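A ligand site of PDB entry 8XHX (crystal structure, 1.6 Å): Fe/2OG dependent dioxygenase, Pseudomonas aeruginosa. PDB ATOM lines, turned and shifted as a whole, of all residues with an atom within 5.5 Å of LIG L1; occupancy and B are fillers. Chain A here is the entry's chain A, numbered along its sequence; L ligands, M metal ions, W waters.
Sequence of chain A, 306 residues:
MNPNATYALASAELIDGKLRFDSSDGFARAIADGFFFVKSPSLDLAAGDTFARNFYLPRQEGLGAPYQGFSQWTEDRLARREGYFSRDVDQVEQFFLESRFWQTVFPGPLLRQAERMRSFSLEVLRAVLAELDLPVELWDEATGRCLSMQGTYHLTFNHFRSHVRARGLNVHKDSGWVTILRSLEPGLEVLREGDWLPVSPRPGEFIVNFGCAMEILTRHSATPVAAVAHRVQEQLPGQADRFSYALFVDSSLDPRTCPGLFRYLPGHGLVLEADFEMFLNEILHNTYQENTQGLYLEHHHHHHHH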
ATOM      1  N   ARG A  81       2.631  17.392  -4.617  1.00  0.00           N
ATOM      2  CA  ARG A  81       2.655  18.823  -4.903  1.00  0.00           C
ATOM      3  C   ARG A  81       4.066  19.425  -4.846  1.00  0.00           C
ATOM      4  O   ARG A  81       4.212  20.622  -5.078  1.00  0.00           O
ATOM      5  CB  ARG A  81       1.729  19.623  -3.968  1.00  0.00           C
ATOM      6  CG  ARG A  81       0.252  19.191  -4.004  1.00  0.00           C
ATOM      7  CD  ARG A  81      -0.579  19.900  -2.924  1.00  0.00           C
ATOM      8  NE  ARG A  81      -0.093  19.544  -1.591  1.00  0.00           N
ATOM      9  CZ  ARG A  81      -0.623  18.598  -0.827  1.00  0.00           C
ATOM     10  NH1 ARG A  81      -1.705  17.940  -1.224  1.00  0.00           N
ATOM     11  NH2 ARG A  81      -0.084  18.328   0.353  1.00  0.00           N
ATOM     12  N   GLU A  82       5.089  18.631  -4.568  1.00  0.00           N
ATOM     13  CA  GLU A  82       6.446  19.148  -4.401  1.00  0.00           C
ATOM     14  C   GLU A  82       7.278  18.890  -5.650  1.00  0.00           C
ATOM     15  O   GLU A  82       7.051  17.923  -6.389  1.00  0.00           O
ATOM     16  CB  GLU A  82       7.126  18.523  -3.180  1.00  0.00           C
ATOM     17  CG  GLU A  82       6.369  18.773  -1.882  1.00  0.00           C
ATOM     18  CD  GLU A  82       6.205  20.252  -1.583  1.00  0.00           C
ATOM     19  OE1 GLU A  82       7.166  21.015  -1.785  1.00  0.00           O
ATOM     20  OE2 GLU A  82       5.104  20.659  -1.152  1.00  0.00           O
ATOM     21  N   GLN A  94       7.853  25.144 -13.164  1.00  0.00           N
ATOM     22  CA  GLN A  94       7.916  25.585 -11.773  1.00  0.00           C
ATOM     23  C   GLN A  94       8.748  24.626 -10.936  1.00  0.00           C
ATOM     24  O   GLN A  94       8.902  23.451 -11.255  1.00  0.00           O
ATOM     25  CB  GLN A  94       6.511  25.678 -11.183  1.00  0.00           C
ATOM     26  CG  GLN A  94       5.657  26.753 -11.841  1.00  0.00           C
ATOM     27  CD  GLN A  94       4.204  26.655 -11.418  1.00  0.00           C
ATOM     28  OE1 GLN A  94       3.601  25.579 -11.501  1.00  0.00           O
ATOM     29  NE2 GLN A  94       3.643  27.762 -10.942  1.00  0.00           N
ATOM     30  N   PHE A  96       8.507  23.828  -6.772  1.00  0.00           N
ATOM     31  CA  PHE A  96       7.921  24.046  -5.450  1.00  0.00           C
ATOM     32  C   PHE A  96       8.757  23.299  -4.429  1.00  0.00           C
ATOM     33  O   PHE A  96       9.029  22.100  -4.612  1.00  0.00           O
ATOM     34  CB  PHE A  96       6.504  23.488  -5.362  1.00  0.00           C
ATOM     35  CG  PHE A  96       5.498  24.129  -6.286  1.00  0.00           C
ATOM     36  CD1 PHE A  96       5.475  23.821  -7.640  1.00  0.00           C
ATOM     37  CD2 PHE A  96       4.526  24.970  -5.772  1.00  0.00           C
ATOM     38  CE1 PHE A  96       4.539  24.399  -8.475  1.00  0.00           C
ATOM     39  CE2 PHE A  96       3.565  25.538  -6.592  1.00  0.00           C
ATOM     40  CZ  PHE A  96       3.569  25.249  -7.957  1.00  0.00           C
ATOM     41  N   THR A 152       3.377  25.356   6.672  1.00  0.00           N
ATOM     42  CA  THR A 152       3.788  24.949   5.338  1.00  0.00           C
ATOM     43  C   THR A 152       4.435  26.167   4.699  1.00  0.00           C
ATOM     44  O   THR A 152       3.750  27.163   4.423  1.00  0.00           O
ATOM     45  CB  THR A 152       2.586  24.483   4.518  1.00  0.00           C
ATOM     46  OG1 THR A 152       1.979  23.345   5.156  1.00  0.00           O
ATOM     47  CG2 THR A 152       2.994  24.110   3.122  1.00  0.00           C
ATOM     48  N   HIS A 154       6.647  27.323   1.485  1.00  0.00           N
ATOM     49  CA  HIS A 154       7.249  26.995   0.199  1.00  0.00           C
ATOM     50  C   HIS A 154       8.126  28.140  -0.272  1.00  0.00           C
ATOM     51  O   HIS A 154       7.739  29.304  -0.185  1.00  0.00           O
ATOM     52  CB  HIS A 154       6.190  26.739  -0.872  1.00  0.00           C
ATOM     53  CG  HIS A 154       5.538  25.400  -0.764  1.00  0.00           C
ATOM     54  ND1 HIS A 154       4.426  25.174   0.025  1.00  0.00           N
ATOM     55  CD2 HIS A 154       5.829  24.214  -1.343  1.00  0.00           C
ATOM     56  CE1 HIS A 154       4.062  23.908  -0.081  1.00  0.00           C
ATOM     57  NE2 HIS A 154       4.903  23.295  -0.899  1.00  0.00           N
ATOM     58  N   THR A 156       9.002  28.834  -3.948  1.00  0.00           N
ATOM     59  CA  THR A 156       8.479  28.329  -5.219  1.00  0.00           C
ATOM     60  C   THR A 156       8.928  29.239  -6.346  1.00  0.00           C
ATOM     61  O   THR A 156       8.809  30.464  -6.234  1.00  0.00           O
ATOM     62  CB  THR A 156       6.957  28.232  -5.173  1.00  0.00           C
ATOM     63  OG1 THR A 156       6.577  27.175  -4.291  1.00  0.00           O
ATOM     64  CG2 THR A 156       6.396  27.946  -6.575  1.00  0.00           C
ATOM     65  N   ASN A 158       9.004  30.295 -10.534  1.00  0.00           N
ATOM     66  CA  ASN A 158       8.325  30.345 -11.827  1.00  0.00           C
ATOM     67  C   ASN A 158       9.361  30.707 -12.881  1.00  0.00           C
ATOM     68  O   ASN A 158      10.001  31.760 -12.762  1.00  0.00           O
ATOM     69  CB  ASN A 158       7.223  31.404 -11.847  1.00  0.00           C
ATOM     70  CG  ASN A 158       6.079  31.089 -10.915  1.00  0.00           C
ATOM     71  OD1 ASN A 158       5.497  30.010 -10.985  1.00  0.00           O
ATOM     72  ND2 ASN A 158       5.755  32.040 -10.053  1.00  0.00           N
ATOM     73  N   LEU A 169       0.687  32.953 -16.481  1.00  0.00           N
ATOM     74  CA  LEU A 169       0.222  32.201 -15.322  1.00  0.00           C
ATOM     75  C   LEU A 169      -1.248  32.522 -15.154  1.00  0.00           C
ATOM     76  O   LEU A 169      -1.624  33.702 -15.148  1.00  0.00           O
ATOM     77  CB  LEU A 169       1.016  32.571 -14.067  1.00  0.00           C
ATOM     78  CG  LEU A 169       0.572  31.907 -12.751  1.00  0.00           C
ATOM     79  CD1 LEU A 169       0.632  30.403 -12.884  1.00  0.00           C
ATOM     80  CD2 LEU A 169       1.437  32.375 -11.597  1.00  0.00           C
ATOM     81  N   HIS A 172      -5.572  33.331 -10.465  1.00  0.00           N
ATOM     82  CA  HIS A 172      -5.635  32.530  -9.243  1.00  0.00           C
ATOM     83  C   HIS A 172      -5.636  33.450  -8.025  1.00  0.00           C
ATOM     84  O   HIS A 172      -5.275  34.627  -8.109  1.00  0.00           O
ATOM     85  CB  HIS A 172      -4.454  31.557  -9.149  1.00  0.00           C
ATOM     86  CG  HIS A 172      -3.130  32.252  -8.977  1.00  0.00           C
ATOM     87  ND1 HIS A 172      -2.451  32.837 -10.026  1.00  0.00           N
ATOM     88  CD2 HIS A 172      -2.380  32.467  -7.870  1.00  0.00           C
ATOM     89  CE1 HIS A 172      -1.332  33.376  -9.571  1.00  0.00           C
ATOM     90  NE2 HIS A 172      -1.264  33.165  -8.267  1.00  0.00           N
ATOM     91  N   LYS A 173      -6.010  32.870  -6.895  1.00  0.00           N
ATOM     92  CA  LYS A 173      -5.643  33.407  -5.592  1.00  0.00           C
ATOM     93  C   LYS A 173      -4.612  32.482  -4.986  1.00  0.00           C
ATOM     94  O   LYS A 173      -4.646  31.274  -5.241  1.00  0.00           O
ATOM     95  CB  LYS A 173      -6.865  33.501  -4.668  1.00  0.00           C
ATOM     96  CG  LYS A 173      -7.850  34.599  -5.049  1.00  0.00           C
ATOM     97  CD  LYS A 173      -9.096  34.540  -4.136  1.00  0.00           C
ATOM     98  CE  LYS A 173     -10.100  35.636  -4.475  1.00  0.00           C
ATOM     99  NZ  LYS A 173     -11.311  35.531  -3.592  1.00  0.00           N
ATOM    100  N   ASP A 174      -3.658  33.042  -4.247  1.00  0.00           N
ATOM    101  CA  ASP A 174      -2.742  32.211  -3.484  1.00  0.00           C
ATOM    102  C   ASP A 174      -3.510  31.538  -2.342  1.00  0.00           C
ATOM    103  O   ASP A 174      -4.545  32.036  -1.881  1.00  0.00           O
ATOM    104  CB  ASP A 174      -1.589  33.032  -2.908  1.00  0.00           C
ATOM    105  CG  ASP A 174      -0.676  33.619  -3.977  1.00  0.00           C
ATOM    106  OD1 ASP A 174      -0.830  33.334  -5.189  1.00  0.00           O
ATOM    107  OD2 ASP A 174       0.231  34.387  -3.589  1.00  0.00           O
ATOM    108  N   SER A 175      -3.004  30.393  -1.879  1.00  0.00           N
ATOM    109  CA  SER A 175      -3.803  29.585  -0.953  1.00  0.00           C
ATOM    110  C   SER A 175      -3.752  30.102   0.486  1.00  0.00           C
ATOM    111  O   SER A 175      -4.709  29.868   1.243  1.00  0.00           O
ATOM    112  CB  SER A 175      -3.323  28.131  -0.971  1.00  0.00           C
ATOM    113  OG  SER A 175      -1.947  28.042  -0.609  1.00  0.00           O
ATOM    114  N   GLY A 176      -2.690  30.795   0.876  1.00  0.00           N
ATOM    115  CA  GLY A 176      -2.391  30.909   2.299  1.00  0.00           C
ATOM    116  C   GLY A 176      -2.513  32.253   2.974  1.00  0.00           C
ATOM    117  O   GLY A 176      -3.508  32.956   2.800  1.00  0.00           O
ATOM    118  N   PHE A 248       5.831  31.402   0.155  1.00  0.00           N
ATOM    119  CA  PHE A 248       4.412  31.244   0.462  1.00  0.00           C
ATOM    120  C   PHE A 248       4.272  30.698   1.869  1.00  0.00           C
ATOM    121  O   PHE A 248       4.834  29.651   2.174  1.00  0.00           O
ATOM    122  CB  PHE A 248       3.731  30.273  -0.519  1.00  0.00           C
ATOM    123  CG  PHE A 248       3.697  30.752  -1.944  1.00  0.00           C
ATOM    124  CD1 PHE A 248       2.561  31.363  -2.448  1.00  0.00           C
ATOM    125  CD2 PHE A 248       4.790  30.576  -2.777  1.00  0.00           C
ATOM    126  CE1 PHE A 248       2.520  31.802  -3.770  1.00  0.00           C
ATOM    127  CE2 PHE A 248       4.761  31.020  -4.096  1.00  0.00           C
ATOM    128  CZ  PHE A 248       3.615  31.630  -4.590  1.00  0.00           C
ATOM    129  N   ASP A 250       1.705  29.077   4.512  1.00  0.00           N
ATOM    130  CA  ASP A 250       0.448  28.343   4.585  1.00  0.00           C
ATOM    131  C   ASP A 250       0.342  27.639   5.929  1.00  0.00           C
ATOM    132  O   ASP A 250       1.335  27.449   6.648  1.00  0.00           O
ATOM    133  CB  ASP A 250       0.340  27.315   3.425  1.00  0.00           C
ATOM    134  CG  ASP A 250      -0.120  27.951   2.110  1.00  0.00           C
ATOM    135  OD1 ASP A 250      -1.339  28.116   1.937  1.00  0.00           O
ATOM    136  OD2 ASP A 250       0.736  28.306   1.268  1.00  0.00           O
ATOM    137  N   PHE A 276      -8.293  21.870   4.755  1.00  0.00           N
ATOM    138  CA  PHE A 276      -7.309  22.654   4.005  1.00  0.00           C
ATOM    139  C   PHE A 276      -6.701  21.839   2.859  1.00  0.00           C
ATOM    140  O   PHE A 276      -6.573  22.355   1.739  1.00  0.00           O
ATOM    141  CB  PHE A 276      -6.217  23.174   4.940  1.00  0.00           C
ATOM    142  CG  PHE A 276      -5.120  23.913   4.214  1.00  0.00           C
ATOM    143  CD1 PHE A 276      -5.423  24.835   3.236  1.00  0.00           C
ATOM    144  CD2 PHE A 276      -3.783  23.667   4.516  1.00  0.00           C
ATOM    145  CE1 PHE A 276      -4.413  25.501   2.553  1.00  0.00           C
ATOM    146  CE2 PHE A 276      -2.774  24.329   3.842  1.00  0.00           C
ATOM    147  CZ  PHE A 276      -3.092  25.237   2.856  1.00  0.00           C
ATOM    148  N   LEU A 280      -6.776  23.020  -0.936  1.00  0.00           N
ATOM    149  CA  LEU A 280      -5.549  23.262  -1.682  1.00  0.00           C
ATOM    150  C   LEU A 280      -5.487  22.401  -2.943  1.00  0.00           C
ATOM    151  O   LEU A 280      -5.141  22.896  -4.028  1.00  0.00           O
ATOM    152  CB  LEU A 280      -4.352  22.980  -0.762  1.00  0.00           C
ATOM    153  CG  LEU A 280      -2.951  23.026  -1.362  1.00  0.00           C
ATOM    154  CD1 LEU A 280      -2.668  24.426  -1.894  1.00  0.00           C
ATOM    155  CD2 LEU A 280      -1.912  22.634  -0.323  1.00  0.00           C
ATOM    156  N   LEU A 284      -5.331  24.259  -6.580  1.00  0.00           N
ATOM    157  CA  LEU A 284      -4.126  24.000  -7.363  1.00  0.00           C
ATOM    158  C   LEU A 284      -4.476  23.372  -8.710  1.00  0.00           C
ATOM    159  O   LEU A 284      -4.005  23.822  -9.759  1.00  0.00           O
ATOM    160  CB  LEU A 284      -3.196  23.082  -6.563  1.00  0.00           C
ATOM    161  CG  LEU A 284      -1.828  22.736  -7.147  1.00  0.00           C
ATOM    162  CD1 LEU A 284      -0.978  24.000  -7.237  1.00  0.00           C
ATOM    163  CD2 LEU A 284      -1.144  21.679  -6.263  1.00  0.00           C
ATOM    164  N   THR A 287      -6.008  25.775 -11.115  1.00  0.00           N
ATOM    165  CA  THR A 287      -5.161  26.845 -11.626  1.00  0.00           C
ATOM    166  C   THR A 287      -4.563  26.490 -12.993  1.00  0.00           C
ATOM    167  O   THR A 287      -4.333  27.383 -13.815  1.00  0.00           O
ATOM    168  CB  THR A 287      -4.066  27.150 -10.606  1.00  0.00           C
ATOM    169  OG1 THR A 287      -4.665  27.653  -9.401  1.00  0.00           O
ATOM    170  CG2 THR A 287      -3.105  28.209 -11.111  1.00  0.00           C
ATOM    171  N   TYR A 288      -4.360  25.207 -13.281  1.00  0.00           N
ATOM    172  CA  TYR A 288      -3.527  24.811 -14.408  1.00  0.00           C
ATOM    173  C   TYR A 288      -4.303  24.073 -15.507  1.00  0.00           C
ATOM    174  O   TYR A 288      -3.675  23.503 -16.406  1.00  0.00           O
ATOM    175  CB  TYR A 288      -2.324  24.000 -13.918  1.00  0.00           C
ATOM    176  CG  TYR A 288      -1.450  24.874 -13.032  1.00  0.00           C
ATOM    177  CD1 TYR A 288      -0.706  25.905 -13.596  1.00  0.00           C
ATOM    178  CD2 TYR A 288      -1.430  24.723 -11.648  1.00  0.00           C
ATOM    179  CE1 TYR A 288       0.057  26.757 -12.812  1.00  0.00           C
ATOM    180  CE2 TYR A 288      -0.674  25.582 -10.849  1.00  0.00           C
ATOM    181  CZ  TYR A 288       0.069  26.585 -11.450  1.00  0.00           C
ATOM    182  OH  TYR A 288       0.805  27.451 -10.673  1.00  0.00           O
HETATM  183  C1  LIG L   1       1.820  27.377  -2.248  1.00  0.00           C
HETATM  184  C2  LIG L   1       2.796  27.732  -3.357  1.00  0.00           C
HETATM  185  C3  LIG L   1       0.987  28.903  -4.788  1.00  0.00           C
HETATM  186  C4  LIG L   1       0.095  28.789  -3.562  1.00  0.00           C
HETATM  187  C5  LIG L   1       0.405  28.025  -5.902  1.00  0.00           C
HETATM  188  C6  LIG L   1       1.676  25.851  -2.144  1.00  0.00           C
HETATM  189  C7  LIG L   1       0.462  28.638  -7.308  1.00  0.00           C
HETATM  190  C8  LIG L   1       1.898  28.928  -7.738  1.00  0.00           C
HETATM  191  C9  LIG L   1      -0.364  29.917  -7.402  1.00  0.00           C
HETATM  192  C10 LIG L   1       0.825  25.523  -0.908  1.00  0.00           C
HETATM  193  C11 LIG L   1       1.056  25.286  -3.410  1.00  0.00           C
HETATM  194  C12 LIG L   1       0.927  23.756  -3.375  1.00  0.00           C
HETATM  195  N1  LIG L   1       0.520  28.046  -2.359  1.00  0.00           N
HETATM  196  N2  LIG L   1       2.372  28.470  -4.529  1.00  0.00           N
HETATM  197  O1  LIG L   1      -0.965  29.343  -3.592  1.00  0.00           O
HETATM  198  O2  LIG L   1       3.948  27.415  -3.233  1.00  0.00           O
HETATM  199  O3  LIG L   1      -0.071  27.704  -8.197  1.00  0.00           O
HETATM  200  O4  LIG L   1       2.165  23.137  -3.201  1.00  0.00           O
HETATM  201  C1  LG2 L   2       2.533  33.066  -7.941  1.00  0.00           C
HETATM  202  O1  LG2 L   2       3.559  32.372  -8.141  1.00  0.00           O
HETATM  203  O2  LG2 L   2       1.613  32.696  -7.181  1.00  0.00           O
HETATM  204  C2  LG2 L   2       2.401  34.344  -8.612  1.00  0.00           C
HETATM  205  O3  LG2 L   2       1.347  34.944  -8.484  1.00  0.00           O
HETATM  206  C3  LG2 L   2       3.555  34.878  -9.445  1.00  0.00           C
HETATM  207  C4  LG2 L   2       3.369  36.346  -9.871  1.00  0.00           C
HETATM  208  C5  LG2 L   2       4.515  36.887 -10.713  1.00  0.00           C
HETATM  209  O4  LG2 L   2       4.671  38.133 -10.752  1.00  0.00           O
HETATM  210  O5  LG2 L   2       5.229  36.091 -11.366  1.00  0.00           O
HETATM  211 FE    FE M   1       0.122  34.107  -6.945  1.00  0.00          FE
HETATM  212  O   HOH W   1       2.504  22.383  -6.094  1.00  0.00           O
HETATM  213  O   HOH W   2      -0.053  30.561  -0.245  1.00  0.00           O
HETATM  214  O   HOH W   3      -2.655  27.350  -7.407  1.00  0.00           O
HETATM  215  O   HOH W   4      -3.323  28.749  -5.071  1.00  0.00           O
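An oxygen (O1) of LIG L1 is in hydrogen-bond range of the backbone NH (N) of Ser 175, 2.9 Å away. N1 of LIG L1 lies within hydrogen-bond range of OG of Ser 175, at 3.0 Å. O1 of LG2 L2 lies within hydrogen-bond range of ND2 of Asn 158. An oxygen (O2) of LIG L1 lies within hydrogen-bond range of the side-chain hydroxyl of Thr 156 (2.8 Å). O3 of LIG L1 lies within hydrogen-bond range of OH of Tyr 288 (2.6 Å).
O of His 154 lies within hydrogen-bond range of N of Phe 248, 2.9 Å away. NE2 of Gln 94 sits at hydrogen-bond distance from OD1 of Asn 158. OG of Ser 175 sits at hydrogen-bond distance from OD1 of Asp 250, 2.6 Å away. A ring nitrogen (NE2) of His 154 lies within hydrogen-bond range of the side-chain carboxylate (OE2) of Glu 82 (2.7 Å). The side-chain hydroxyl (OH) of Tyr 288 is in hydrogen-bond range of the side-chain amide nitrogen (NE2) of Gln 94. N of Asp 250 sits at hydrogen-bond distance from O of Thr 152 (2.8 Å). The side-chain carboxylate (OD1) of Asp 250 lies close to the backbone NH (N) of Gly 176, 3.2 Å away.
CB of Arg 81 touches O4 of LIG L1 (3.6 Å). Gln 94 touches LIG L1 (NE2 to C8, 3.8 Å). CD2 of Phe 96 touches O2 of LIG L1, 3.6 Å away. His 154 touches LIG L1 (CB to O2, 3.3 Å). His 172 touches LIG L1. Asp 174 touches LIG L1 (CA to O1, 3.4 Å). Phe 248 touches LIG L1. OD2 of Asp 250 touches C10 of LIG L1, at 3.5 Å. Leu 280 touches LIG L1. Leu 284 touches LIG L1. Hydrophobic or aromatic side chains within 4 Å of LIG L1: Phe 96, His 154, His 172, Phe 248, Leu 280, Leu 284 and Tyr 288. Within 4 Å of LIG L1: Arg 81, Gln 94, Phe 96, His 154, Thr 156, His 172, Asp 174, Ser 175, Phe 248, Asp 250, Leu 280, Leu 284 and Tyr 288.
Water W3 lies within hydrogen-bond range of O3 of LIG L1 (2.7 Å) and OG1 of Thr 287 (2.8 Å). Water W4 lies within hydrogen-bond range of an oxygen (O1) of LIG L1 and the backbone carbonyl oxygen of Lys 173. Water W1 lies within hydrogen-bond range of O of Arg 81 (2.7 Å) and O4 of LIG L1 (3.0 Å). Water W2 lies within hydrogen-bond range of OD2 of Asp 250 (2.8 Å), N of Gly 176 (2.9 Å), OG of Ser 175 (3.2 Å) and N1 of LIG L1 (3.3 Å).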
